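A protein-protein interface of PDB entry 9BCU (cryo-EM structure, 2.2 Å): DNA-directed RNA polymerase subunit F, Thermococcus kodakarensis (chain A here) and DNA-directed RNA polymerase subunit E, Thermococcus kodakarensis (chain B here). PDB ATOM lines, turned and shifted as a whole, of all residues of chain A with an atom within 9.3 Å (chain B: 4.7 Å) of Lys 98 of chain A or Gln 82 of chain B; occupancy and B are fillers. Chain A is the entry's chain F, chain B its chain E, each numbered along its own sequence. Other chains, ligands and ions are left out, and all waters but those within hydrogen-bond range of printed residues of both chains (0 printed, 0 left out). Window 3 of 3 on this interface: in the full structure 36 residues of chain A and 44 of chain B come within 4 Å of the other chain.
Of chain A, only Lys 98 (3.5 Å) comes within 4 Å of Gln 82 of chain B. No residue of chain A comes within 4 Å of Asn 81 of chain B. Of the printed residues of chain A, Val 84 of chain B touches Lys 80 (3.2 Å) and Ile 95 (3.6 Å). Of the printed residues of chain A, Arg 145 of chain B touches Val 94 (2.9 Å), Ile 95 (3.8 Å) and Lys 98 (3.7 Å). Of the printed residues of chain A, Glu 83 of chain B touches Lys 80 (2.9 Å). Of the printed residues of chain B, Arg 76 of chain A touches Arg 80. Printed residues of chain A within 4 Å of Arg 80 of chain B: Arg 76. Ile 146 of chain B touches none of the printed residues of chain A. The nearest residue of chain A that does not touch Gln 82 of chain B is Glu 99 of chain A (5.6 Å).
Of the 16 printed residues of chain A, 5 touch a printed residue of chain B. Hydrophobic or aromatic side chains of chain A within 4 Å of the printed part of chain B: Ile 95. Of the 8 printed residues of chain B, 5 touch a printed residue of chain A. Printed residues of chain B that touch a printed residue of chain A: Arg 80, Gln 82, Glu 83, Val 84 and Arg 145. Among the printed residues, 8 pairs touch across the chains.
The guanidinium group (NH1) of Arg 76 of chain A is in salt-bridge range of the side-chain carboxylate (OE2) of Glu 99 of chain A (2.9 Å). The backbone carbonyl oxygen (O) of Glu 83 of chain B sits at hydrogen-bond distance from the backbone NH (N) of Ile 146 of chain B (2.8 Å). NE of Arg 145 of chain B lies within hydrogen-bond range of O of Gln 82 of chain B, at 3.5 Å. The side-chain carboxylate (OE1) of Glu 83 of chain B lies within hydrogen-bond range of the backbone NH (N) of Arg 80 of chain B, at 3.3 Å. O of Ile 146 of chain B is in hydrogen-bond range of N of Gln 82 of chain B (2.9 Å).
O of Val 94 of chain A sits at hydrogen-bond distance from NH1 of Arg 145 of chain B. The backbone carbonyl oxygen (O) of Val 84 of chain B lies close to the side-chain amino group (NZ) of Lys 80 of chain A, at 3.4 Å. The side-chain carboxylate (OE2) of Glu 83 of chain B lies within salt-bridge range of the side-chain amino group (NZ) of Lys 80 of chain A, at 2.9 Å.
CD of Arg 76 of chain A touches NE of Arg 80 of chain B (3.5 Å). CG2 of Val 84 of chain B touches CG2 of Ile 95 of chain A (3.6 Å). NH2 of Arg 145 of chain B touches CA of Ile 95 of chain A, 3.8 Å away. CE of Lys 98 of chain A touches OE1 of Gln 82 of chain B, 3.5 Å away. Lys 98 of chain A touches Arg 145 of chain B.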
ATOM      1  N   ARG A  76       8.586  13.628   8.905  1.00  0.00           N
ATOM      2  CA  ARG A  76       9.082  13.170  10.200  1.00  0.00           C
ATOM      3  C   ARG A  76       8.889  11.667  10.371  1.00  0.00           C
ATOM      4  O   ARG A  76       9.837  10.939  10.693  1.00  0.00           O
ATOM      5  CB  ARG A  76       8.384  13.935  11.325  1.00  0.00           C
ATOM      6  CG  ARG A  76       8.504  13.282  12.691  1.00  0.00           C
ATOM      7  CD  ARG A  76       7.614  13.970  13.712  1.00  0.00           C
ATOM      8  NE  ARG A  76       6.327  14.351  13.144  1.00  0.00           N
ATOM      9  CZ  ARG A  76       5.188  13.712  13.371  1.00  0.00           C
ATOM     10  NH1 ARG A  76       5.139  12.646  14.155  1.00  0.00           N
ATOM     11  NH2 ARG A  76       4.072  14.151  12.799  1.00  0.00           N
ATOM     12  N   ILE A  77       7.669  11.176  10.144  1.00  0.00           N
ATOM     13  CA  ILE A  77       7.429   9.749  10.311  1.00  0.00           C
ATOM     14  C   ILE A  77       8.047   8.941   9.178  1.00  0.00           C
ATOM     15  O   ILE A  77       8.370   7.766   9.372  1.00  0.00           O
ATOM     16  CB  ILE A  77       5.923   9.457  10.462  1.00  0.00           C
ATOM     17  CG1 ILE A  77       5.192   9.570   9.124  1.00  0.00           C
ATOM     18  CG2 ILE A  77       5.301  10.387  11.495  1.00  0.00           C
ATOM     19  CD1 ILE A  77       3.723   9.227   9.221  1.00  0.00           C
ATOM     20  N   LYS A  80      11.429   8.510  10.448  1.00  0.00           N
ATOM     21  CA  LYS A  80      11.340   7.548  11.542  1.00  0.00           C
ATOM     22  C   LYS A  80      11.260   6.119  11.017  1.00  0.00           C
ATOM     23  O   LYS A  80      11.909   5.214  11.554  1.00  0.00           O
ATOM     24  CB  LYS A  80      10.128   7.866  12.416  1.00  0.00           C
ATOM     25  CG  LYS A  80      10.000   6.991  13.649  1.00  0.00           C
ATOM     26  CD  LYS A  80      11.269   7.042  14.481  1.00  0.00           C
ATOM     27  CE  LYS A  80      11.296   8.284  15.354  1.00  0.00           C
ATOM     28  NZ  LYS A  80      12.680   8.795  15.552  1.00  0.00           N
ATOM     29  N   ASP A  91       5.574  -3.785  14.753  1.00  0.00           N
ATOM     30  CA  ASP A  91       6.344  -2.569  15.001  1.00  0.00           C
ATOM     31  C   ASP A  91       5.696  -1.353  14.349  1.00  0.00           C
ATOM     32  O   ASP A  91       5.590  -0.291  14.974  1.00  0.00           O
ATOM     33  CB  ASP A  91       7.781  -2.742  14.510  1.00  0.00           C
ATOM     34  CG  ASP A  91       7.865  -3.518  13.213  1.00  0.00           C
ATOM     35  OD1 ASP A  91       6.925  -3.418  12.400  1.00  0.00           O
ATOM     36  OD2 ASP A  91       8.875  -4.222  13.005  1.00  0.00           O
ATOM     37  N   ILE A  92       5.255  -1.482  13.096  1.00  0.00           N
ATOM     38  CA  ILE A  92       4.593  -0.358  12.442  1.00  0.00           C
ATOM     39  C   ILE A  92       3.274  -0.041  13.140  1.00  0.00           C
ATOM     40  O   ILE A  92       2.897   1.130  13.276  1.00  0.00           O
ATOM     41  CB  ILE A  92       4.411  -0.632  10.934  1.00  0.00           C
ATOM     42  CG1 ILE A  92       3.673   0.524  10.254  1.00  0.00           C
ATOM     43  CG2 ILE A  92       3.692  -1.940  10.688  1.00  0.00           C
ATOM     44  CD1 ILE A  92       3.771   0.507   8.745  1.00  0.00           C
ATOM     45  N   ARG A  93       2.579  -1.068  13.636  1.00  0.00           N
ATOM     46  CA  ARG A  93       1.347  -0.839  14.384  1.00  0.00           C
ATOM     47  C   ARG A  93       1.612  -0.053  15.665  1.00  0.00           C
ATOM     48  O   ARG A  93       0.892   0.903  15.978  1.00  0.00           O
ATOM     49  CB  ARG A  93       0.675  -2.175  14.703  1.00  0.00           C
ATOM     50  CG  ARG A  93      -0.588  -2.050  15.540  1.00  0.00           C
ATOM     51  CD  ARG A  93      -0.736  -3.224  16.493  1.00  0.00           C
ATOM     52  NE  ARG A  93      -1.142  -4.442  15.802  1.00  0.00           N
ATOM     53  CZ  ARG A  93      -2.398  -4.851  15.678  1.00  0.00           C
ATOM     54  NH1 ARG A  93      -3.402  -4.160  16.193  1.00  0.00           N
ATOM     55  NH2 ARG A  93      -2.651  -5.981  15.025  1.00  0.00           N
ATOM     56  N   VAL A  94       2.649  -0.432  16.415  1.00  0.00           N
ATOM     57  CA  VAL A  94       2.902   0.244  17.685  1.00  0.00           C
ATOM     58  C   VAL A  94       3.552   1.610  17.499  1.00  0.00           C
ATOM     59  O   VAL A  94       3.508   2.434  18.421  1.00  0.00           O
ATOM     60  CB  VAL A  94       3.758  -0.612  18.635  1.00  0.00           C
ATOM     61  CG1 VAL A  94       3.067  -1.938  18.929  1.00  0.00           C
ATOM     62  CG2 VAL A  94       5.151  -0.831  18.074  1.00  0.00           C
ATOM     63  N   ILE A  95       4.157   1.884  16.340  1.00  0.00           N
ATOM     64  CA  ILE A  95       4.653   3.236  16.091  1.00  0.00           C
ATOM     65  C   ILE A  95       3.621   4.126  15.406  1.00  0.00           C
ATOM     66  O   ILE A  95       3.796   5.353  15.383  1.00  0.00           O
ATOM     67  CB  ILE A  95       5.951   3.234  15.261  1.00  0.00           C
ATOM     68  CG1 ILE A  95       5.674   2.811  13.817  1.00  0.00           C
ATOM     69  CG2 ILE A  95       7.007   2.355  15.914  1.00  0.00           C
ATOM     70  CD1 ILE A  95       6.865   2.962  12.899  1.00  0.00           C
ATOM     71  N   PHE A  96       2.555   3.552  14.847  1.00  0.00           N
ATOM     72  CA  PHE A  96       1.483   4.341  14.256  1.00  0.00           C
ATOM     73  C   PHE A  96       0.260   4.471  15.155  1.00  0.00           C
ATOM     74  O   PHE A  96      -0.634   5.263  14.840  1.00  0.00           O
ATOM     75  CB  PHE A  96       1.058   3.737  12.912  1.00  0.00           C
ATOM     76  CG  PHE A  96       1.644   4.436  11.719  1.00  0.00           C
ATOM     77  CD1 PHE A  96       1.103   5.628  11.265  1.00  0.00           C
ATOM     78  CD2 PHE A  96       2.733   3.903  11.052  1.00  0.00           C
ATOM     79  CE1 PHE A  96       1.638   6.275  10.166  1.00  0.00           C
ATOM     80  CE2 PHE A  96       3.274   4.544   9.953  1.00  0.00           C
ATOM     81  CZ  PHE A  96       2.725   5.731   9.510  1.00  0.00           C
ATOM     82  N   ALA A  97       0.192   3.706  16.250  1.00  0.00           N
ATOM     83  CA  ALA A  97      -0.955   3.803  17.149  1.00  0.00           C
ATOM     84  C   ALA A  97      -1.051   5.182  17.791  1.00  0.00           C
ATOM     85  O   ALA A  97      -2.147   5.742  17.913  1.00  0.00           O
ATOM     86  CB  ALA A  97      -0.872   2.718  18.222  1.00  0.00           C
ATOM     87  N   LYS A  98       0.080   5.747  18.204  1.00  0.00           N
ATOM     88  CA  LYS A  98       0.096   7.054  18.846  1.00  0.00           C
ATOM     89  C   LYS A  98       0.123   8.206  17.850  1.00  0.00           C
ATOM     90  O   LYS A  98       0.084   9.367  18.269  1.00  0.00           O
ATOM     91  CB  LYS A  98       1.296   7.165  19.795  1.00  0.00           C
ATOM     92  CG  LYS A  98       1.335   6.096  20.886  1.00  0.00           C
ATOM     93  CD  LYS A  98       0.451   6.424  22.095  1.00  0.00           C
ATOM     94  CE  LYS A  98       0.238   7.920  22.300  1.00  0.00           C
ATOM     95  NZ  LYS A  98      -0.354   8.221  23.633  1.00  0.00           N
ATOM     96  N   GLU A  99       0.187   7.918  16.553  1.00  0.00           N
ATOM     97  CA  GLU A  99       0.171   8.960  15.542  1.00  0.00           C
ATOM     98  C   GLU A  99      -1.263   9.425  15.288  1.00  0.00           C
ATOM     99  O   GLU A  99      -2.225   8.918  15.872  1.00  0.00           O
ATOM    100  CB  GLU A  99       0.825   8.462  14.255  1.00  0.00           C
ATOM    101  CG  GLU A  99       2.342   8.437  14.301  1.00  0.00           C
ATOM    102  CD  GLU A  99       2.953   9.818  14.169  1.00  0.00           C
ATOM    103  OE1 GLU A  99       2.305  10.702  13.569  1.00  0.00           O
ATOM    104  OE2 GLU A  99       4.080  10.021  14.667  1.00  0.00           O
ATOM    105  N   GLU A 100      -1.408  10.407  14.399  1.00  0.00           N
ATOM    106  CA  GLU A 100      -2.718  10.952  14.070  1.00  0.00           C
ATOM    107  C   GLU A 100      -3.537  10.038  13.167  1.00  0.00           C
ATOM    108  O   GLU A 100      -4.733  10.288  12.986  1.00  0.00           O
ATOM    109  CB  GLU A 100      -2.563  12.325  13.408  1.00  0.00           C
ATOM    110  CG  GLU A 100      -2.393  12.280  11.896  1.00  0.00           C
ATOM    111  CD  GLU A 100      -1.063  11.687  11.475  1.00  0.00           C
ATOM    112  OE1 GLU A 100      -0.059  11.913  12.183  1.00  0.00           O
ATOM    113  OE2 GLU A 100      -1.022  10.994  10.437  1.00  0.00           O
ATOM    114  N   TYR A 101      -2.934   8.992  12.606  1.00  0.00           N
ATOM    115  CA  TYR A 101      -3.621   8.095  11.691  1.00  0.00           C
ATOM    116  C   TYR A 101      -3.384   6.650  12.105  1.00  0.00           C
ATOM    117  O   TYR A 101      -2.356   6.314  12.700  1.00  0.00           O
ATOM    118  CB  TYR A 101      -3.158   8.309  10.242  1.00  0.00           C
ATOM    119  CG  TYR A 101      -3.988   7.574   9.213  1.00  0.00           C
ATOM    120  CD1 TYR A 101      -5.373   7.682   9.206  1.00  0.00           C
ATOM    121  CD2 TYR A 101      -3.389   6.773   8.250  1.00  0.00           C
ATOM    122  CE1 TYR A 101      -6.138   7.014   8.268  1.00  0.00           C
ATOM    123  CE2 TYR A 101      -4.145   6.102   7.307  1.00  0.00           C
ATOM    124  CZ  TYR A 101      -5.518   6.225   7.321  1.00  0.00           C
ATOM    125  OH  TYR A 101      -6.274   5.557   6.385  1.00  0.00           O
ATOM    126  N   MET A 102      -4.355   5.794  11.781  1.00  0.00           N
ATOM    127  CA  MET A 102      -4.318   4.363  12.083  1.00  0.00           C
ATOM    128  C   MET A 102      -4.481   3.625  10.761  1.00  0.00           C
ATOM    129  O   MET A 102      -5.605   3.266  10.376  1.00  0.00           O
ATOM    130  CB  MET A 102      -5.419   3.985  13.073  1.00  0.00           C
ATOM    131  CG  MET A 102      -5.240   2.709  13.931  1.00  0.00           C
ATOM    132  SD  MET A 102      -3.699   2.377  14.837  1.00  0.00           S
ATOM    133  CE  MET A 102      -2.571   1.752  13.590  1.00  0.00           C
ATOM    134  N   PRO A 103      -3.393   3.384  10.030  1.00  0.00           N
ATOM    135  CA  PRO A 103      -3.521   2.816   8.683  1.00  0.00           C
ATOM    136  C   PRO A 103      -3.933   1.352   8.698  1.00  0.00           C
ATOM    137  O   PRO A 103      -3.594   0.592   9.609  1.00  0.00           O
ATOM    138  CB  PRO A 103      -2.117   2.993   8.084  1.00  0.00           C
ATOM    139  CG  PRO A 103      -1.205   3.333   9.224  1.00  0.00           C
ATOM    140  CD  PRO A 103      -1.996   3.439  10.488  1.00  0.00           C
ATOM    141  N   ARG B  80      10.757  14.333  21.123  1.00  0.00           N
ATOM    142  CA  ARG B  80       9.341  14.643  21.216  1.00  0.00           C
ATOM    143  C   ARG B  80       8.616  13.554  21.996  1.00  0.00           C
ATOM    144  O   ARG B  80       9.099  12.426  22.128  1.00  0.00           O
ATOM    145  CB  ARG B  80       8.712  14.800  19.825  1.00  0.00           C
ATOM    146  CG  ARG B  80       9.373  13.965  18.743  1.00  0.00           C
ATOM    147  CD  ARG B  80       9.396  14.706  17.417  1.00  0.00           C
ATOM    148  NE  ARG B  80       8.057  15.087  16.984  1.00  0.00           N
ATOM    149  CZ  ARG B  80       7.729  16.291  16.536  1.00  0.00           C
ATOM    150  NH1 ARG B  80       8.622  17.264  16.451  1.00  0.00           N
ATOM    151  NH2 ARG B  80       6.474  16.525  16.164  1.00  0.00           N
ATOM    152  N   ASN B  81       7.449  13.913  22.521  1.00  0.00           N
ATOM    153  CA  ASN B  81       6.644  12.972  23.285  1.00  0.00           C
ATOM    154  C   ASN B  81       6.085  11.879  22.381  1.00  0.00           C
ATOM    155  O   ASN B  81       5.756  12.114  21.215  1.00  0.00           O
ATOM    156  CB  ASN B  81       5.502  13.700  23.995  1.00  0.00           C
ATOM    157  CG  ASN B  81       5.258  13.175  25.394  1.00  0.00           C
ATOM    158  OD1 ASN B  81       6.015  12.346  25.899  1.00  0.00           O
ATOM    159  ND2 ASN B  81       4.196  13.656  26.030  1.00  0.00           N
ATOM    160  N   GLN B  82       5.981  10.671  22.943  1.00  0.00           N
ATOM    161  CA  GLN B  82       5.456   9.495  22.243  1.00  0.00           C
ATOM    162  C   GLN B  82       6.239   9.206  20.964  1.00  0.00           C
ATOM    163  O   GLN B  82       5.667   8.864  19.927  1.00  0.00           O
ATOM    164  CB  GLN B  82       3.961   9.647  21.946  1.00  0.00           C
ATOM    165  CG  GLN B  82       3.131  10.059  23.150  1.00  0.00           C
ATOM    166  CD  GLN B  82       3.255   9.086  24.305  1.00  0.00           C
ATOM    167  OE1 GLN B  82       3.188   7.871  24.118  1.00  0.00           O
ATOM    168  NE2 GLN B  82       3.435   9.616  25.509  1.00  0.00           N
ATOM    169  N   GLU B  83       7.559   9.344  21.038  1.00  0.00           N
ATOM    170  CA  GLU B  83       8.445   9.094  19.910  1.00  0.00           C
ATOM    171  C   GLU B  83       9.308   7.875  20.204  1.00  0.00           C
ATOM    172  O   GLU B  83       9.981   7.820  21.237  1.00  0.00           O
ATOM    173  CB  GLU B  83       9.327  10.312  19.623  1.00  0.00           C
ATOM    174  CG  GLU B  83      10.193  10.170  18.383  1.00  0.00           C
ATOM    175  CD  GLU B  83      11.484  10.958  18.480  1.00  0.00           C
ATOM    176  OE1 GLU B  83      11.685  11.648  19.501  1.00  0.00           O
ATOM    177  OE2 GLU B  83      12.297  10.888  17.535  1.00  0.00           O
ATOM    178  N   VAL B  84       9.281   6.907  19.296  1.00  0.00           N
ATOM    179  CA  VAL B  84      10.057   5.682  19.449  1.00  0.00           C
ATOM    180  C   VAL B  84      11.503   5.944  19.054  1.00  0.00           C
ATOM    181  O   VAL B  84      11.780   6.578  18.030  1.00  0.00           O
ATOM    182  CB  VAL B  84       9.444   4.550  18.607  1.00  0.00           C
ATOM    183  CG1 VAL B  84       8.279   3.912  19.345  1.00  0.00           C
ATOM    184  CG2 VAL B  84       8.989   5.091  17.261  1.00  0.00           C
ATOM    185  N   ARG B 145      10.283   4.032  23.674  1.00  0.00           N
ATOM    186  CA  ARG B 145       9.483   5.178  23.267  1.00  0.00           C
ATOM    187  C   ARG B 145       9.523   6.235  24.362  1.00  0.00           C
ATOM    188  O   ARG B 145       9.264   5.932  25.531  1.00  0.00           O
ATOM    189  CB  ARG B 145       8.038   4.764  22.975  1.00  0.00           C
ATOM    190  CG  ARG B 145       7.025   5.891  23.095  1.00  0.00           C
ATOM    191  CD  ARG B 145       5.624   5.411  22.758  1.00  0.00           C
ATOM    192  NE  ARG B 145       5.263   5.716  21.379  1.00  0.00           N
ATOM    193  CZ  ARG B 145       4.807   4.826  20.509  1.00  0.00           C
ATOM    194  NH1 ARG B 145       4.644   3.555  20.841  1.00  0.00           N
ATOM    195  NH2 ARG B 145       4.509   5.219  19.274  1.00  0.00           N
ATOM    196  N   ILE B 146       9.840   7.472  23.977  1.00  0.00           N
ATOM    197  CA  ILE B 146       9.956   8.562  24.939  1.00  0.00           C
ATOM    198  C   ILE B 146       8.575   8.937  25.459  1.00  0.00           C
ATOM    199  O   ILE B 146       7.623   9.094  24.684  1.00  0.00           O
ATOM    200  CB  ILE B 146      10.654   9.771  24.300  1.00  0.00           C
ATOM    201  CG1 ILE B 146      11.942   9.337  23.597  1.00  0.00           C
ATOM    202  CG2 ILE B 146      10.943  10.837  25.345  1.00  0.00           C
ATOM    203  CD1 ILE B 146      12.576  10.428  22.764  1.00  0.00           C
ATOM    204  N   ILE B 147       8.461   9.080  26.777  1.00  0.00           N
ATOM    205  CA  ILE B 147       7.212   9.498  27.406  1.00  0.00           C
ATOM    206  C   ILE B 147       7.361  10.756  28.246  1.00  0.00           C
ATOM    207  O   ILE B 147       6.341  11.322  28.667  1.00  0.00           O
ATOM    208  CB  ILE B 147       6.603   8.366  28.261  1.00  0.00           C
ATOM    209  CG1 ILE B 147       7.666   7.755  29.175  1.00  0.00           C
ATOM    210  CG2 ILE B 147       5.982   7.301  27.371  1.00  0.00           C
ATOM    211  CD1 ILE B 147       7.100   6.846  30.244  1.00  0.00           C
